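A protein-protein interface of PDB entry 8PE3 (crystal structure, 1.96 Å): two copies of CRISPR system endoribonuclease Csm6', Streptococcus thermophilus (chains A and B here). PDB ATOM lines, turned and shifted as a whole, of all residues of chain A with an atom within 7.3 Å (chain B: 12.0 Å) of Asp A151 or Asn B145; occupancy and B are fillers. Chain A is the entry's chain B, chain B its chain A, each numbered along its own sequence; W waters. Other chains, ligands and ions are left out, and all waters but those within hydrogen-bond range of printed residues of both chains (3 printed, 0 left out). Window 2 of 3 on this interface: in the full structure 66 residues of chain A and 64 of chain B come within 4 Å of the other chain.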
ATOM      1  N   ASP A  14       6.153 -15.640   9.160  1.00  0.00           N
ATOM      2  CA  ASP A  14       7.057 -15.117  10.182  1.00  0.00           C
ATOM      3  C   ASP A  14       6.579 -15.448  11.596  1.00  0.00           C
ATOM      4  O   ASP A  14       7.398 -15.532  12.520  1.00  0.00           O
ATOM      5  CB  ASP A  14       7.223 -13.603  10.030  1.00  0.00           C
ATOM      6  CG  ASP A  14       7.975 -13.212   8.757  1.00  0.00           C
ATOM      7  OD1 ASP A  14       7.457 -12.379   7.986  1.00  0.00           O
ATOM      8  OD2 ASP A  14       9.058 -13.785   8.490  1.00  0.00           O
ATOM      9  N   ASN A  52      13.785 -25.244  12.714  1.00  0.00           N
ATOM     10  CA  ASN A  52      12.967 -24.846  13.857  1.00  0.00           C
ATOM     11  C   ASN A  52      11.518 -25.255  13.656  1.00  0.00           C
ATOM     12  O   ASN A  52      10.833 -25.659  14.608  1.00  0.00           O
ATOM     13  CB  ASN A  52      13.062 -23.335  14.076  1.00  0.00           C
ATOM     14  CG  ASN A  52      14.337 -22.923  14.791  1.00  0.00           C
ATOM     15  OD1 ASN A  52      15.191 -23.758  15.101  1.00  0.00           O
ATOM     16  ND2 ASN A  52      14.479 -21.625  15.044  1.00  0.00           N
ATOM     17  N   GLY A 147       6.466  -8.237  18.533  1.00  0.00           N
ATOM     18  CA  GLY A 147       7.596  -8.609  17.710  1.00  0.00           C
ATOM     19  C   GLY A 147       7.561 -10.071  17.296  1.00  0.00           C
ATOM     20  O   GLY A 147       6.703 -10.853  17.712  1.00  0.00           O
ATOM     21  N   HIS A 148       8.533 -10.443  16.465  1.00  0.00           N
ATOM     22  CA  HIS A 148       8.656 -11.807  15.965  1.00  0.00           C
ATOM     23  C   HIS A 148       9.809 -12.527  16.656  1.00  0.00           C
ATOM     24  O   HIS A 148      10.908 -11.976  16.785  1.00  0.00           O
ATOM     25  CB  HIS A 148       8.837 -11.816  14.447  1.00  0.00           C
ATOM     26  CG  HIS A 148       7.678 -11.223  13.710  1.00  0.00           C
ATOM     27  ND1 HIS A 148       6.602 -11.976  13.288  1.00  0.00           N
ATOM     28  CD2 HIS A 148       7.424  -9.952  13.316  1.00  0.00           C
ATOM     29  CE1 HIS A 148       5.734 -11.195  12.670  1.00  0.00           C
ATOM     30  NE2 HIS A 148       6.209  -9.963  12.673  1.00  0.00           N
ATOM     31  N   ASP A 149       9.549 -13.763  17.088  1.00  0.00           N
ATOM     32  CA  ASP A 149      10.471 -14.536  17.907  1.00  0.00           C
ATOM     33  C   ASP A 149      11.401 -15.420  17.085  1.00  0.00           C
ATOM     34  O   ASP A 149      11.876 -16.448  17.589  1.00  0.00           O
ATOM     35  CB  ASP A 149       9.683 -15.390  18.904  1.00  0.00           C
ATOM     36  CG  ASP A 149       8.759 -14.563  19.778  1.00  0.00           C
ATOM     37  OD1 ASP A 149       8.935 -13.323  19.791  1.00  0.00           O
ATOM     38  OD2 ASP A 149       7.869 -15.146  20.450  1.00  0.00           O
ATOM     39  N   ASN A 150      11.683 -15.067  15.834  1.00  0.00           N
ATOM     40  CA  ASN A 150      12.462 -15.988  15.017  1.00  0.00           C
ATOM     41  C   ASN A 150      13.939 -15.958  15.354  1.00  0.00           C
ATOM     42  O   ASN A 150      14.674 -16.872  14.960  1.00  0.00           O
ATOM     43  CB  ASN A 150      12.264 -15.688  13.535  1.00  0.00           C
ATOM     44  CG  ASN A 150      10.916 -16.125  13.046  1.00  0.00           C
ATOM     45  OD1 ASN A 150      10.512 -17.276  13.246  1.00  0.00           O
ATOM     46  ND2 ASN A 150      10.191 -15.207  12.418  1.00  0.00           N
ATOM     47  N   ASP A 151      14.388 -14.941  16.076  1.00  0.00           N
ATOM     48  CA  ASP A 151      15.787 -14.808  16.437  1.00  0.00           C
ATOM     49  C   ASP A 151      16.053 -15.301  17.852  1.00  0.00           C
ATOM     50  O   ASP A 151      17.166 -15.137  18.361  1.00  0.00           O
ATOM     51  CB  ASP A 151      16.208 -13.353  16.275  1.00  0.00           C
ATOM     52  CG  ASP A 151      16.261 -12.941  14.822  1.00  0.00           C
ATOM     53  OD1 ASP A 151      16.723 -13.759  13.996  1.00  0.00           O
ATOM     54  OD2 ASP A 151      15.803 -11.820  14.502  1.00  0.00           O
ATOM     55  N   GLU A 152      15.055 -15.915  18.482  1.00  0.00           N
ATOM     56  CA  GLU A 152      15.103 -16.372  19.857  1.00  0.00           C
ATOM     57  C   GLU A 152      15.529 -17.839  19.891  1.00  0.00           C
ATOM     58  O   GLU A 152      15.715 -18.487  18.857  1.00  0.00           O
ATOM     59  CB  GLU A 152      13.735 -16.172  20.513  1.00  0.00           C
ATOM     60  CG  GLU A 152      13.331 -14.710  20.650  1.00  0.00           C
ATOM     61  CD  GLU A 152      13.939 -14.014  21.859  1.00  0.00           C
ATOM     62  OE1 GLU A 152      13.951 -14.613  22.959  1.00  0.00           O
ATOM     63  OE2 GLU A 152      14.414 -12.866  21.698  1.00  0.00           O
ATOM     64  N   ASN A 153      15.682 -18.378  21.097  1.00  0.00           N
ATOM     65  CA  ASN A 153      16.094 -19.767  21.231  1.00  0.00           C
ATOM     66  C   ASN A 153      14.890 -20.677  21.046  1.00  0.00           C
ATOM     67  O   ASN A 153      13.880 -20.534  21.743  1.00  0.00           O
ATOM     68  CB  ASN A 153      16.739 -20.022  22.592  1.00  0.00           C
ATOM     69  CG  ASN A 153      17.161 -21.465  22.761  1.00  0.00           C
ATOM     70  OD1 ASN A 153      16.405 -22.295  23.267  1.00  0.00           O
ATOM     71  ND2 ASN A 153      18.369 -21.777  22.311  1.00  0.00           N
ATOM     72  N   ILE A 154      15.003 -21.622  20.111  1.00  0.00           N
ATOM     73  CA  ILE A 154      13.857 -22.462  19.779  1.00  0.00           C
ATOM     74  C   ILE A 154      13.468 -23.322  20.972  1.00  0.00           C
ATOM     75  O   ILE A 154      12.280 -23.533  21.245  1.00  0.00           O
ATOM     76  CB  ILE A 154      14.156 -23.307  18.524  1.00  0.00           C
ATOM     77  CG1 ILE A 154      12.893 -24.027  18.043  1.00  0.00           C
ATOM     78  CG2 ILE A 154      15.288 -24.288  18.776  1.00  0.00           C
ATOM     79  CD1 ILE A 154      11.662 -23.126  17.971  1.00  0.00           C
ATOM     80  N   LEU A 157      11.712 -21.013  23.454  1.00  0.00           N
ATOM     81  CA  LEU A 157      10.355 -20.818  22.950  1.00  0.00           C
ATOM     82  C   LEU A 157       9.475 -22.030  23.232  1.00  0.00           C
ATOM     83  O   LEU A 157       8.350 -21.894  23.729  1.00  0.00           O
ATOM     84  CB  LEU A 157      10.402 -20.526  21.450  1.00  0.00           C
ATOM     85  CG  LEU A 157      11.009 -19.183  21.034  1.00  0.00           C
ATOM     86  CD1 LEU A 157      11.079 -19.053  19.519  1.00  0.00           C
ATOM     87  CD2 LEU A 157      10.205 -18.038  21.628  1.00  0.00           C
ATOM     88  N   THR B  15      -0.494   0.161   8.857  1.00  0.00           N
ATOM     89  CA  THR B  15       0.585   0.743   8.075  1.00  0.00           C
ATOM     90  C   THR B  15       0.180   2.083   7.467  1.00  0.00           C
ATOM     91  O   THR B  15       1.034   2.804   6.939  1.00  0.00           O
ATOM     92  CB  THR B  15       1.015  -0.281   7.004  1.00  0.00           C
ATOM     93  OG1 THR B  15       1.480  -1.467   7.659  1.00  0.00           O
ATOM     94  CG2 THR B  15       2.136   0.231   6.113  1.00  0.00           C
ATOM     95  N   ARG B  19       4.715   4.479   7.277  1.00  0.00           N
ATOM     96  CA  ARG B  19       5.487   3.470   7.982  1.00  0.00           C
ATOM     97  C   ARG B  19       6.885   3.451   7.395  1.00  0.00           C
ATOM     98  O   ARG B  19       7.047   3.534   6.171  1.00  0.00           O
ATOM     99  CB  ARG B  19       4.850   2.085   7.863  1.00  0.00           C
ATOM    100  CG  ARG B  19       5.495   1.022   8.738  1.00  0.00           C
ATOM    101  CD  ARG B  19       4.593  -0.193   8.833  1.00  0.00           C
ATOM    102  NE  ARG B  19       5.217  -1.323   9.509  1.00  0.00           N
ATOM    103  CZ  ARG B  19       4.879  -2.586   9.288  1.00  0.00           C
ATOM    104  NH1 ARG B  19       3.988  -2.908   8.368  1.00  0.00           N
ATOM    105  NH2 ARG B  19       5.457  -3.547  10.001  1.00  0.00           N
ATOM    106  N   ASN B  20       7.886   3.376   8.275  1.00  0.00           N
ATOM    107  CA  ASN B  20       9.275   3.155   7.877  1.00  0.00           C
ATOM    108  C   ASN B  20       9.736   4.174   6.833  1.00  0.00           C
ATOM    109  O   ASN B  20      10.266   3.825   5.772  1.00  0.00           O
ATOM    110  CB  ASN B  20       9.454   1.728   7.365  1.00  0.00           C
ATOM    111  CG  ASN B  20      10.896   1.314   7.299  1.00  0.00           C
ATOM    112  OD1 ASN B  20      11.734   1.831   8.039  1.00  0.00           O
ATOM    113  ND2 ASN B  20      11.201   0.363   6.419  1.00  0.00           N
ATOM    114  N   PHE B  21       9.508   5.455   7.140  1.00  0.00           N
ATOM    115  CA  PHE B  21       9.932   6.562   6.283  1.00  0.00           C
ATOM    116  C   PHE B  21       9.290   6.502   4.907  1.00  0.00           C
ATOM    117  O   PHE B  21       9.855   7.006   3.933  1.00  0.00           O
ATOM    118  CB  PHE B  21      11.456   6.610   6.131  1.00  0.00           C
ATOM    119  CG  PHE B  21      12.186   6.725   7.428  1.00  0.00           C
ATOM    120  CD1 PHE B  21      12.458   5.608   8.195  1.00  0.00           C
ATOM    121  CD2 PHE B  21      12.595   7.955   7.887  1.00  0.00           C
ATOM    122  CE1 PHE B  21      13.124   5.724   9.393  1.00  0.00           C
ATOM    123  CE2 PHE B  21      13.259   8.077   9.084  1.00  0.00           C
ATOM    124  CZ  PHE B  21      13.525   6.960   9.837  1.00  0.00           C
ATOM    125  N   SER B 137       6.023  -3.249  -0.026  1.00  0.00           N
ATOM    126  CA  SER B 137       6.835  -2.719   1.055  1.00  0.00           C
ATOM    127  C   SER B 137       8.071  -2.040   0.472  1.00  0.00           C
ATOM    128  O   SER B 137       8.631  -2.518  -0.525  1.00  0.00           O
ATOM    129  CB  SER B 137       7.263  -3.827   2.017  1.00  0.00           C
ATOM    130  OG  SER B 137       8.104  -3.304   3.035  1.00  0.00           O
ATOM    131  N   PRO B 138       8.520  -0.926   1.053  1.00  0.00           N
ATOM    132  CA  PRO B 138       9.818  -0.368   0.643  1.00  0.00           C
ATOM    133  C   PRO B 138      10.975  -1.306   0.935  1.00  0.00           C
ATOM    134  O   PRO B 138      12.055  -1.141   0.349  1.00  0.00           O
ATOM    135  CB  PRO B 138       9.916   0.927   1.458  1.00  0.00           C
ATOM    136  CG  PRO B 138       9.094   0.647   2.685  1.00  0.00           C
ATOM    137  CD  PRO B 138       7.962  -0.233   2.228  1.00  0.00           C
ATOM    138  N   GLU B 139      10.782  -2.286   1.823  1.00  0.00           N
ATOM    139  CA  GLU B 139      11.789  -3.315   2.040  1.00  0.00           C
ATOM    140  C   GLU B 139      11.869  -4.309   0.897  1.00  0.00           C
ATOM    141  O   GLU B 139      12.882  -5.001   0.772  1.00  0.00           O
ATOM    142  CB  GLU B 139      11.498  -4.082   3.319  1.00  0.00           C
ATOM    143  CG  GLU B 139      11.522  -3.225   4.535  1.00  0.00           C
ATOM    144  CD  GLU B 139      12.920  -2.731   4.861  1.00  0.00           C
ATOM    145  OE1 GLU B 139      13.760  -3.558   5.287  1.00  0.00           O
ATOM    146  OE2 GLU B 139      13.170  -1.512   4.709  1.00  0.00           O
ATOM    147  N   ALA B 141      10.624  -7.070   0.770  1.00  0.00           N
ATOM    148  CA  ALA B 141      10.886  -8.273   1.547  1.00  0.00           C
ATOM    149  C   ALA B 141       9.910  -8.238   2.716  1.00  0.00           C
ATOM    150  O   ALA B 141       9.110  -7.306   2.842  1.00  0.00           O
ATOM    151  CB  ALA B 141      12.337  -8.330   2.025  1.00  0.00           C
ATOM    152  N   SER B 142       9.988  -9.247   3.577  1.00  0.00           N
ATOM    153  CA  SER B 142       9.154  -9.270   4.771  1.00  0.00           C
ATOM    154  C   SER B 142       9.349  -7.995   5.593  1.00  0.00           C
ATOM    155  O   SER B 142      10.453  -7.451   5.674  1.00  0.00           O
ATOM    156  CB  SER B 142       9.491 -10.505   5.607  1.00  0.00           C
ATOM    157  OG  SER B 142       9.000 -10.398   6.929  1.00  0.00           O
ATOM    158  N   ASN B 143       8.259  -7.493   6.182  1.00  0.00           N
ATOM    159  CA  ASN B 143       8.346  -6.400   7.147  1.00  0.00           C
ATOM    160  C   ASN B 143       8.644  -6.893   8.555  1.00  0.00           C
ATOM    161  O   ASN B 143       8.423  -6.153   9.520  1.00  0.00           O
ATOM    162  CB  ASN B 143       7.055  -5.569   7.166  1.00  0.00           C
ATOM    163  CG  ASN B 143       6.869  -4.730   5.913  1.00  0.00           C
ATOM    164  OD1 ASN B 143       7.808  -4.099   5.421  1.00  0.00           O
ATOM    165  ND2 ASN B 143       5.647  -4.711   5.396  1.00  0.00           N
ATOM    166  N   GLU B 144       9.096  -8.134   8.701  1.00  0.00           N
ATOM    167  CA  GLU B 144       9.537  -8.611  10.002  1.00  0.00           C
ATOM    168  C   GLU B 144      10.620  -7.688  10.535  1.00  0.00           C
ATOM    169  O   GLU B 144      11.452  -7.177   9.773  1.00  0.00           O
ATOM    170  CB  GLU B 144      10.066 -10.039   9.887  1.00  0.00           C
ATOM    171  CG  GLU B 144      10.467 -10.679  11.187  1.00  0.00           C
ATOM    172  CD  GLU B 144      11.348 -11.893  10.971  1.00  0.00           C
ATOM    173  OE1 GLU B 144      12.033 -11.957   9.925  1.00  0.00           O
ATOM    174  OE2 GLU B 144      11.353 -12.784  11.847  1.00  0.00           O
ATOM    175  N   ASN B 145      10.586  -7.442  11.847  1.00  0.00           N
ATOM    176  CA  ASN B 145      11.597  -6.625  12.512  1.00  0.00           C
ATOM    177  C   ASN B 145      11.494  -5.156  12.095  1.00  0.00           C
ATOM    178  O   ASN B 145      12.482  -4.418  12.132  1.00  0.00           O
ATOM    179  CB  ASN B 145      13.007  -7.167  12.231  1.00  0.00           C
ATOM    180  CG  ASN B 145      13.284  -8.485  12.942  1.00  0.00           C
ATOM    181  OD1 ASN B 145      12.623  -8.836  13.929  1.00  0.00           O
ATOM    182  ND2 ASN B 145      14.243  -9.245  12.414  1.00  0.00           N
ATOM    183  N   ILE B 146      10.306  -4.728  11.670  1.00  0.00           N
ATOM    184  CA  ILE B 146      10.056  -3.343  11.282  1.00  0.00           C
ATOM    185  C   ILE B 146       8.777  -2.881  11.959  1.00  0.00           C
ATOM    186  O   ILE B 146       7.709  -3.466  11.743  1.00  0.00           O
ATOM    187  CB  ILE B 146       9.955  -3.170   9.763  1.00  0.00           C
ATOM    188  CG1 ILE B 146      11.351  -3.243   9.161  1.00  0.00           C
ATOM    189  CG2 ILE B 146       9.295  -1.846   9.431  1.00  0.00           C
ATOM    190  CD1 ILE B 146      11.426  -2.653   7.811  1.00  0.00           C
ATOM    191  N   GLY B 147       8.885  -1.824  12.769  1.00  0.00           N
ATOM    192  CA  GLY B 147       7.798  -1.417  13.633  1.00  0.00           C
ATOM    193  C   GLY B 147       6.812  -0.488  12.963  1.00  0.00           C
ATOM    194  O   GLY B 147       6.995  -0.040  11.829  1.00  0.00           O
ATOM    195  N   HIS B 148       5.745  -0.194  13.696  1.00  0.00           N
ATOM    196  CA  HIS B 148       4.678   0.661  13.203  1.00  0.00           C
ATOM    197  C   HIS B 148       4.831   2.072  13.758  1.00  0.00           C
ATOM    198  O   HIS B 148       5.144   2.264  14.938  1.00  0.00           O
ATOM    199  CB  HIS B 148       3.317   0.064  13.564  1.00  0.00           C
ATOM    200  CG  HIS B 148       3.004  -1.188  12.806  1.00  0.00           C
ATOM    201  ND1 HIS B 148       3.175  -2.448  13.343  1.00  0.00           N
ATOM    202  CD2 HIS B 148       2.560  -1.377  11.539  1.00  0.00           C
ATOM    203  CE1 HIS B 148       2.837  -3.357  12.445  1.00  0.00           C
ATOM    204  NE2 HIS B 148       2.459  -2.734  11.342  1.00  0.00           N
ATOM    205  N   ASP B 149       4.618   3.058  12.888  1.00  0.00           N
ATOM    206  CA  ASP B 149       4.844   4.463  13.187  1.00  0.00           C
ATOM    207  C   ASP B 149       3.599   5.159  13.732  1.00  0.00           C
ATOM    208  O   ASP B 149       3.494   6.387  13.636  1.00  0.00           O
ATOM    209  CB  ASP B 149       5.326   5.184  11.923  1.00  0.00           C
ATOM    210  CG  ASP B 149       6.680   4.685  11.453  1.00  0.00           C
ATOM    211  OD1 ASP B 149       7.203   5.203  10.435  1.00  0.00           O
ATOM    212  OD2 ASP B 149       7.205   3.750  12.100  1.00  0.00           O
HETATM  213  O   HOH W   1      12.292 -12.362  14.453  1.00  0.00           O
HETATM  214  O   HOH W   2      10.445  -8.740  15.430  1.00  0.00           O
HETATM  215  O   HOH W   3       6.338 -10.165   8.947  1.00  0.00           O
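The side-chain carboxylate (OD1) of Asp A14 sits at hydrogen-bond distance from the side-chain hydroxyl (OG) of Ser B142, 2.7 Å away.
The side-chain amide nitrogen of Asn A150 sits at hydrogen-bond distance from the side-chain carboxylate of Glu B144, 2.7 Å away.
The side-chain hydroxyl (OG) of Ser B142 sits at hydrogen-bond distance from the backbone NH (N) of Glu B144, at 2.9 Å.
The backbone carbonyl oxygen (O) of Asp A14 lies within hydrogen-bond range of the side-chain amide nitrogen (ND2) of Asn A150.
Among the printed residues, pairs that only touch across the chains: Asp A14 with Glu B144, His A148 with Glu B144 and Asp A151 with Asn B145.
Of the printed residues of chain B, Asp A151 touches Asn B145 (3.7 Å).
Asn B145 touches just one residue of chain A: Asp A151.
Of chain B, only Glu B144 (3.7 Å) comes within 4 Å of His A148.
No residue of chain B comes within 4 Å of Asp A149.
Asn A150 touches just one residue of chain B: Glu B144.
No residue of chain B comes within 4 Å of Glu A152.
Printed residues of chain B within 4 Å of Asp A14: Ser B142 (2.7 Å) and Glu B144 (3.8 Å).
Printed residues of chain A within 4 Å of Glu B144: Asp A14, His A148 and Asn A150.
Of the printed residues of chain A, Ser B142 touches Asp A14 (2.7 Å).
Ile B146 touches none of the printed residues of chain A.
The nearest residue of chain A that does not touch Asn B145 is His A148 (4.3 Å).
The nearest printed residue of chain A that does not touch Ser B142 is His A148 (6.4 Å).
Along chain A the printed residues that touch a printed residue of chain B span positions 14 to 151.
Of the 16 printed residues of chain B, 3 touch a printed residue of chain A.
3 positions are printed for both chains.
Water W2 bridges OD1 of Asn B145 and N of His A148.
Water W3 lies within hydrogen-bond range of the side-chain carboxylate (OD1) of Asp A14 (2.7 Å), the side-chain hydroxyl (OG) of Ser B142 (3.3 Å) and the backbone NH (N) of Glu B144 (3.4 Å).
Water W1 lies within hydrogen-bond range of O of His A148, OE2 of Glu B144 and N of Asn A150.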
